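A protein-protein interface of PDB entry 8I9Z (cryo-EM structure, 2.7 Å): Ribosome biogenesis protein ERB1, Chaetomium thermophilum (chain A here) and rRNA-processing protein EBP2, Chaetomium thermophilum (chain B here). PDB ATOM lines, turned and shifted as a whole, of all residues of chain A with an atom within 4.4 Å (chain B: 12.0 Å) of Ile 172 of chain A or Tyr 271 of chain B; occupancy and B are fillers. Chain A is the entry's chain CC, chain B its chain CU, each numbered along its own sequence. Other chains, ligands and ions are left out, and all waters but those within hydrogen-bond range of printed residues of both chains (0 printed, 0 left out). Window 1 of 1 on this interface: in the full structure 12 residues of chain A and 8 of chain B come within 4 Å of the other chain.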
ATOM      1  N   ASN A 170      25.256 -22.156  10.671  1.00  0.00           N
ATOM      2  CA  ASN A 170      25.051 -20.923  11.418  1.00  0.00           C
ATOM      3  C   ASN A 170      24.073 -21.056  12.580  1.00  0.00           C
ATOM      4  O   ASN A 170      24.155 -20.253  13.513  1.00  0.00           O
ATOM      5  CB  ASN A 170      24.572 -19.814  10.486  1.00  0.00           C
ATOM      6  CG  ASN A 170      24.845 -18.435  11.044  1.00  0.00           C
ATOM      7  OD1 ASN A 170      25.628 -18.278  11.972  1.00  0.00           O
ATOM      8  ND2 ASN A 170      24.196 -17.428  10.479  1.00  0.00           N
ATOM      9  N   THR A 171      23.149 -22.022  12.529  1.00  0.00           N
ATOM     10  CA  THR A 171      22.092 -22.228  13.541  1.00  0.00           C
ATOM     11  C   THR A 171      21.288 -20.957  13.814  1.00  0.00           C
ATOM     12  O   THR A 171      20.830 -20.720  14.929  1.00  0.00           O
ATOM     13  CB  THR A 171      22.646 -22.787  14.855  1.00  0.00           C
ATOM     14  OG1 THR A 171      23.241 -21.729  15.613  1.00  0.00           O
ATOM     15  CG2 THR A 171      23.675 -23.868  14.589  1.00  0.00           C
ATOM     16  N   ILE A 172      21.113 -20.132  12.791  1.00  0.00           N
ATOM     17  CA  ILE A 172      20.352 -18.895  12.880  1.00  0.00           C
ATOM     18  C   ILE A 172      19.135 -19.063  11.986  1.00  0.00           C
ATOM     19  O   ILE A 172      19.271 -19.405  10.804  1.00  0.00           O
ATOM     20  CB  ILE A 172      21.198 -17.682  12.459  1.00  0.00           C
ATOM     21  CG1 ILE A 172      22.359 -17.478  13.431  1.00  0.00           C
ATOM     22  CG2 ILE A 172      20.366 -16.437  12.384  1.00  0.00           C
ATOM     23  CD1 ILE A 172      21.948 -17.458  14.876  1.00  0.00           C
ATOM     24  N   GLY A 173      17.953 -18.838  12.545  1.00  0.00           N
ATOM     25  CA  GLY A 173      16.729 -19.129  11.832  1.00  0.00           C
ATOM     26  C   GLY A 173      16.346 -18.088  10.806  1.00  0.00           C
ATOM     27  O   GLY A 173      17.204 -17.554  10.099  1.00  0.00           O
ATOM     28  N   ILE A 175      15.432 -15.094  11.229  1.00  0.00           N
ATOM     29  CA  ILE A 175      15.546 -13.732  11.737  1.00  0.00           C
ATOM     30  C   ILE A 175      16.340 -12.900  10.738  1.00  0.00           C
ATOM     31  O   ILE A 175      17.137 -13.457   9.968  1.00  0.00           O
ATOM     32  CB  ILE A 175      16.194 -13.705  13.131  1.00  0.00           C
ATOM     33  CG1 ILE A 175      17.633 -14.194  13.062  1.00  0.00           C
ATOM     34  CG2 ILE A 175      15.393 -14.544  14.104  1.00  0.00           C
ATOM     35  CD1 ILE A 175      18.520 -13.591  14.105  1.00  0.00           C
ATOM     36  N   TYR A 180      23.256  -8.694  13.726  1.00  0.00           N
ATOM     37  CA  TYR A 180      24.682  -8.929  13.839  1.00  0.00           C
ATOM     38  C   TYR A 180      25.512  -7.898  13.097  1.00  0.00           C
ATOM     39  O   TYR A 180      26.688  -8.162  12.825  1.00  0.00           O
ATOM     40  CB  TYR A 180      25.038 -10.319  13.298  1.00  0.00           C
ATOM     41  CG  TYR A 180      24.554 -11.471  14.135  1.00  0.00           C
ATOM     42  CD1 TYR A 180      25.189 -11.817  15.317  1.00  0.00           C
ATOM     43  CD2 TYR A 180      23.468 -12.227  13.733  1.00  0.00           C
ATOM     44  CE1 TYR A 180      24.748 -12.876  16.074  1.00  0.00           C
ATOM     45  CE2 TYR A 180      23.022 -13.285  14.484  1.00  0.00           C
ATOM     46  CZ  TYR A 180      23.665 -13.604  15.650  1.00  0.00           C
ATOM     47  OH  TYR A 180      23.214 -14.661  16.397  1.00  0.00           O
ATOM     48  N   GLY A 187      26.398 -15.385  14.306  1.00  0.00           N
ATOM     49  CA  GLY A 187      25.785 -16.612  14.775  1.00  0.00           C
ATOM     50  C   GLY A 187      26.693 -17.488  15.624  1.00  0.00           C
ATOM     51  O   GLY A 187      27.876 -17.222  15.835  1.00  0.00           O
ATOM     52  N   TYR A 188      26.097 -18.573  16.120  1.00  0.00           N
ATOM     53  CA  TYR A 188      26.772 -19.595  16.906  1.00  0.00           C
ATOM     54  C   TYR A 188      26.511 -20.955  16.279  1.00  0.00           C
ATOM     55  O   TYR A 188      25.414 -21.215  15.790  1.00  0.00           O
ATOM     56  CB  TYR A 188      26.264 -19.630  18.354  1.00  0.00           C
ATOM     57  CG  TYR A 188      26.852 -18.609  19.293  1.00  0.00           C
ATOM     58  CD1 TYR A 188      26.512 -17.270  19.198  1.00  0.00           C
ATOM     59  CD2 TYR A 188      27.716 -18.992  20.302  1.00  0.00           C
ATOM     60  CE1 TYR A 188      27.033 -16.343  20.063  1.00  0.00           C
ATOM     61  CE2 TYR A 188      28.243 -18.069  21.173  1.00  0.00           C
ATOM     62  CZ  TYR A 188      27.898 -16.746  21.046  1.00  0.00           C
ATOM     63  OH  TYR A 188      28.424 -15.825  21.917  1.00  0.00           O
ATOM     64  N   PRO B 264      27.419 -25.982  27.440  1.00  0.00           N
ATOM     65  CA  PRO B 264      26.975 -24.601  27.659  1.00  0.00           C
ATOM     66  C   PRO B 264      25.493 -24.528  27.989  1.00  0.00           C
ATOM     67  O   PRO B 264      24.668 -25.219  27.393  1.00  0.00           O
ATOM     68  CB  PRO B 264      27.285 -23.917  26.325  1.00  0.00           C
ATOM     69  CG  PRO B 264      28.346 -24.753  25.708  1.00  0.00           C
ATOM     70  CD  PRO B 264      28.039 -26.156  26.117  1.00  0.00           C
ATOM     71  N   PHE B 265      25.164 -23.673  28.951  1.00  0.00           N
ATOM     72  CA  PHE B 265      23.803 -23.551  29.454  1.00  0.00           C
ATOM     73  C   PHE B 265      23.209 -22.173  29.209  1.00  0.00           C
ATOM     74  O   PHE B 265      22.131 -22.066  28.618  1.00  0.00           O
ATOM     75  CB  PHE B 265      23.782 -23.874  30.956  1.00  0.00           C
ATOM     76  CG  PHE B 265      22.413 -24.140  31.504  1.00  0.00           C
ATOM     77  CD1 PHE B 265      21.880 -25.412  31.476  1.00  0.00           C
ATOM     78  CD2 PHE B 265      21.665 -23.119  32.059  1.00  0.00           C
ATOM     79  CE1 PHE B 265      20.627 -25.659  31.982  1.00  0.00           C
ATOM     80  CE2 PHE B 265      20.411 -23.358  32.564  1.00  0.00           C
ATOM     81  CZ  PHE B 265      19.892 -24.631  32.527  1.00  0.00           C
ATOM     82  N   THR B 266      23.884 -21.116  29.645  1.00  0.00           N
ATOM     83  CA  THR B 266      23.329 -19.771  29.574  1.00  0.00           C
ATOM     84  C   THR B 266      23.409 -19.237  28.152  1.00  0.00           C
ATOM     85  O   THR B 266      24.458 -19.314  27.507  1.00  0.00           O
ATOM     86  CB  THR B 266      24.078 -18.841  30.524  1.00  0.00           C
ATOM     87  OG1 THR B 266      24.135 -19.434  31.826  1.00  0.00           O
ATOM     88  CG2 THR B 266      23.375 -17.497  30.621  1.00  0.00           C
ATOM     89  N   ARG B 267      22.302 -18.698  27.670  1.00  0.00           N
ATOM     90  CA  ARG B 267      22.289 -18.037  26.378  1.00  0.00           C
ATOM     91  C   ARG B 267      23.068 -16.733  26.462  1.00  0.00           C
ATOM     92  O   ARG B 267      22.785 -15.911  27.342  1.00  0.00           O
ATOM     93  CB  ARG B 267      20.855 -17.779  25.931  1.00  0.00           C
ATOM     94  CG  ARG B 267      20.733 -17.144  24.563  1.00  0.00           C
ATOM     95  CD  ARG B 267      19.339 -16.606  24.335  1.00  0.00           C
ATOM     96  NE  ARG B 267      19.085 -16.378  22.920  1.00  0.00           N
ATOM     97  CZ  ARG B 267      18.102 -15.627  22.441  1.00  0.00           C
ATOM     98  NH1 ARG B 267      17.214 -15.065  23.238  1.00  0.00           N
ATOM     99  NH2 ARG B 267      18.006 -15.446  21.129  1.00  0.00           N
ATOM    100  N   PRO B 268      24.053 -16.510  25.599  1.00  0.00           N
ATOM    101  CA  PRO B 268      24.782 -15.241  25.622  1.00  0.00           C
ATOM    102  C   PRO B 268      23.920 -14.088  25.149  1.00  0.00           C
ATOM    103  O   PRO B 268      22.936 -14.267  24.429  1.00  0.00           O
ATOM    104  CB  PRO B 268      25.951 -15.483  24.660  1.00  0.00           C
ATOM    105  CG  PRO B 268      26.007 -16.951  24.467  1.00  0.00           C
ATOM    106  CD  PRO B 268      24.612 -17.438  24.614  1.00  0.00           C
ATOM    107  N   THR B 269      24.308 -12.886  25.570  1.00  0.00           N
ATOM    108  CA  THR B 269      23.588 -11.686  25.176  1.00  0.00           C
ATOM    109  C   THR B 269      23.760 -11.367  23.699  1.00  0.00           C
ATOM    110  O   THR B 269      22.936 -10.644  23.134  1.00  0.00           O
ATOM    111  CB  THR B 269      24.048 -10.500  26.020  1.00  0.00           C
ATOM    112  OG1 THR B 269      25.451 -10.619  26.287  1.00  0.00           O
ATOM    113  CG2 THR B 269      23.293 -10.465  27.335  1.00  0.00           C
ATOM    114  N   ASP B 270      24.806 -11.890  23.061  1.00  0.00           N
ATOM    115  CA  ASP B 270      25.039 -11.690  21.638  1.00  0.00           C
ATOM    116  C   ASP B 270      24.652 -12.911  20.809  1.00  0.00           C
ATOM    117  O   ASP B 270      25.286 -13.193  19.789  1.00  0.00           O
ATOM    118  CB  ASP B 270      26.499 -11.318  21.386  1.00  0.00           C
ATOM    119  CG  ASP B 270      27.459 -12.106  22.252  1.00  0.00           C
ATOM    120  OD1 ASP B 270      28.642 -12.217  21.875  1.00  0.00           O
ATOM    121  OD2 ASP B 270      27.036 -12.612  23.310  1.00  0.00           O
ATOM    122  N   TYR B 271      23.629 -13.650  21.231  1.00  0.00           N
ATOM    123  CA  TYR B 271      23.082 -14.761  20.456  1.00  0.00           C
ATOM    124  C   TYR B 271      21.651 -14.404  20.079  1.00  0.00           C
ATOM    125  O   TYR B 271      20.731 -14.544  20.888  1.00  0.00           O
ATOM    126  CB  TYR B 271      23.133 -16.071  21.237  1.00  0.00           C
ATOM    127  CG  TYR B 271      22.707 -17.266  20.415  1.00  0.00           C
ATOM    128  CD1 TYR B 271      23.057 -17.368  19.078  1.00  0.00           C
ATOM    129  CD2 TYR B 271      21.948 -18.282  20.969  1.00  0.00           C
ATOM    130  CE1 TYR B 271      22.673 -18.445  18.325  1.00  0.00           C
ATOM    131  CE2 TYR B 271      21.560 -19.364  20.219  1.00  0.00           C
ATOM    132  CZ  TYR B 271      21.922 -19.438  18.899  1.00  0.00           C
ATOM    133  OH  TYR B 271      21.540 -20.514  18.143  1.00  0.00           O
ATOM    134  N   PHE B 272      21.468 -13.941  18.850  1.00  0.00           N
ATOM    135  CA  PHE B 272      20.158 -13.612  18.309  1.00  0.00           C
ATOM    136  C   PHE B 272      19.751 -14.732  17.363  1.00  0.00           C
ATOM    137  O   PHE B 272      20.451 -14.997  16.382  1.00  0.00           O
ATOM    138  CB  PHE B 272      20.189 -12.275  17.572  1.00  0.00           C
ATOM    139  CG  PHE B 272      21.000 -11.219  18.258  1.00  0.00           C
ATOM    140  CD1 PHE B 272      20.481 -10.513  19.325  1.00  0.00           C
ATOM    141  CD2 PHE B 272      22.280 -10.927  17.829  1.00  0.00           C
ATOM    142  CE1 PHE B 272      21.224  -9.540  19.954  1.00  0.00           C
ATOM    143  CE2 PHE B 272      23.026  -9.958  18.454  1.00  0.00           C
ATOM    144  CZ  PHE B 272      22.497  -9.263  19.516  1.00  0.00           C
ATOM    145  N   ALA B 273      18.628 -15.385  17.650  1.00  0.00           N
ATOM    146  CA  ALA B 273      18.209 -16.525  16.851  1.00  0.00           C
ATOM    147  C   ALA B 273      16.692 -16.642  16.872  1.00  0.00           C
ATOM    148  O   ALA B 273      16.007 -15.952  17.629  1.00  0.00           O
ATOM    149  CB  ALA B 273      18.854 -17.823  17.342  1.00  0.00           C
ATOM    150  N   GLU B 274      16.181 -17.530  16.022  1.00  0.00           N
ATOM    151  CA  GLU B 274      14.745 -17.749  15.909  1.00  0.00           C
ATOM    152  C   GLU B 274      14.197 -18.395  17.174  1.00  0.00           C
ATOM    153  O   GLU B 274      14.837 -19.256  17.780  1.00  0.00           O
ATOM    154  CB  GLU B 274      14.446 -18.624  14.693  1.00  0.00           C
ATOM    155  CG  GLU B 274      12.975 -18.776  14.353  1.00  0.00           C
ATOM    156  CD  GLU B 274      12.395 -17.539  13.700  1.00  0.00           C
ATOM    157  OE1 GLU B 274      13.156 -16.799  13.043  1.00  0.00           O
ATOM    158  OE2 GLU B 274      11.176 -17.305  13.842  1.00  0.00           O
ATOM    159  N   MET B 275      13.001 -17.970  17.571  1.00  0.00           N
ATOM    160  CA  MET B 275      12.348 -18.455  18.774  1.00  0.00           C
ATOM    161  C   MET B 275      11.011 -19.090  18.410  1.00  0.00           C
ATOM    162  O   MET B 275      10.534 -18.977  17.279  1.00  0.00           O
ATOM    163  CB  MET B 275      12.165 -17.321  19.788  1.00  0.00           C
ATOM    164  CG  MET B 275      13.425 -16.504  20.003  1.00  0.00           C
ATOM    165  SD  MET B 275      14.176 -16.805  21.606  1.00  0.00           S
ATOM    166  CE  MET B 275      13.070 -15.900  22.672  1.00  0.00           C
ATOM    167  N   VAL B 276      10.410 -19.777  19.385  1.00  0.00           N
ATOM    168  CA  VAL B 276       9.171 -20.505  19.123  1.00  0.00           C
ATOM    169  C   VAL B 276       8.000 -19.543  18.956  1.00  0.00           C
ATOM    170  O   VAL B 276       7.048 -19.827  18.222  1.00  0.00           O
ATOM    171  CB  VAL B 276       8.907 -21.551  20.223  1.00  0.00           C
ATOM    172  CG1 VAL B 276       9.973 -22.624  20.185  1.00  0.00           C
ATOM    173  CG2 VAL B 276       8.855 -20.918  21.596  1.00  0.00           C
ATOM    174  N   ASP B 279       8.512 -12.271  17.347  1.00  0.00           N
ATOM    175  CA  ASP B 279       8.627 -10.961  17.978  1.00  0.00           C
ATOM    176  C   ASP B 279       7.322 -10.189  17.873  1.00  0.00           C
ATOM    177  O   ASP B 279       7.023  -9.341  18.720  1.00  0.00           O
ATOM    178  CB  ASP B 279       9.765 -10.167  17.342  1.00  0.00           C
ATOM    179  CG  ASP B 279      11.128 -10.652  17.776  1.00  0.00           C
ATOM    180  OD1 ASP B 279      11.221 -11.786  18.289  1.00  0.00           O
ATOM    181  OD2 ASP B 279      12.108  -9.901  17.603  1.00  0.00           O
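Asn 170 of chain A touches none of the printed residues of chain B. Thr 171 of chain A touches just one residue of chain B: Tyr 271 (3.3 Å). Ile 172 of chain A touches just these residues of chain B: Tyr 271 (3.7 Å), Phe 272 (3.3 Å) and Ala 273 (3.97 Å). Of chain B, only Phe 272, Ala 273 and Glu 274 come within 4 Å of Ile 175 of chain A. No residue of chain B comes within 4 Å of Gly 187 of chain A. Tyr 271 of chain B touches just these residues of chain A: Thr 171, Ile 172, Tyr 180 and Tyr 188. Printed residues of chain A within 4 Å of Phe 272 of chain B: Ile 172 (3.3 Å), Ile 175 (3.3 Å) and Tyr 180 (2.8 Å). Of the printed residues of chain A, Ala 273 of chain B touches Ile 172 and Ile 175. Printed residues of chain A within 4 Å of Glu 274 of chain B: Gly 173 (3.7 Å) and Ile 175 (3.3 Å). The nearest printed residue of chain A that does not touch Tyr 271 of chain B is Gly 187 of chain A (4.9 Å).
OH of Tyr 180 of chain A is in hydrogen-bond range of O of Phe 272 of chain B. The side-chain hydroxyl (OH) of Tyr 271 of chain B is in hydrogen-bond range of the side-chain hydroxyl (OG1) of Thr 171 of chain A (3.3 Å). OE1 of Glu 274 of chain B sits close to N of Ile 175 of chain A (3.4 Å).
The backbone carbonyl oxygen of Tyr 271 of chain B is in hydrogen-bond range of the guanidinium group of Arg 267 of chain B (2.9 Å).
Among the printed residues, merely in contact across the chains: Ile 172 of chain A with Tyr 271 of chain B, Ile 172 of chain A with Phe 272 of chain B, Ile 172 of chain A with Ala 273 of chain B, Gly 173 of chain A with Glu 274 of chain B, Ile 175 of chain A with Phe 272 of chain B, Ile 175 of chain A with Ala 273 of chain B, Tyr 180 of chain A with Asp 270 of chain B, Tyr 180 of chain A with Tyr 271 of chain B, Tyr 188 of chain A with Pro 268 of chain B, Tyr 188 of chain A with Asp 270 of chain B and Tyr 188 of chain A with Tyr 271 of chain B.
Printed residues of chain A that touch a printed residue of chain B: Thr 171, Ile 172, Gly 173, Ile 175, Tyr 180 and Tyr 188. Hydrophobic or aromatic side chains of chain A that line the printed part of chain B: Ile 172, Ile 175, Tyr 180 and Tyr 188. Among the printed residues, 14 pairs touch across the chains.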
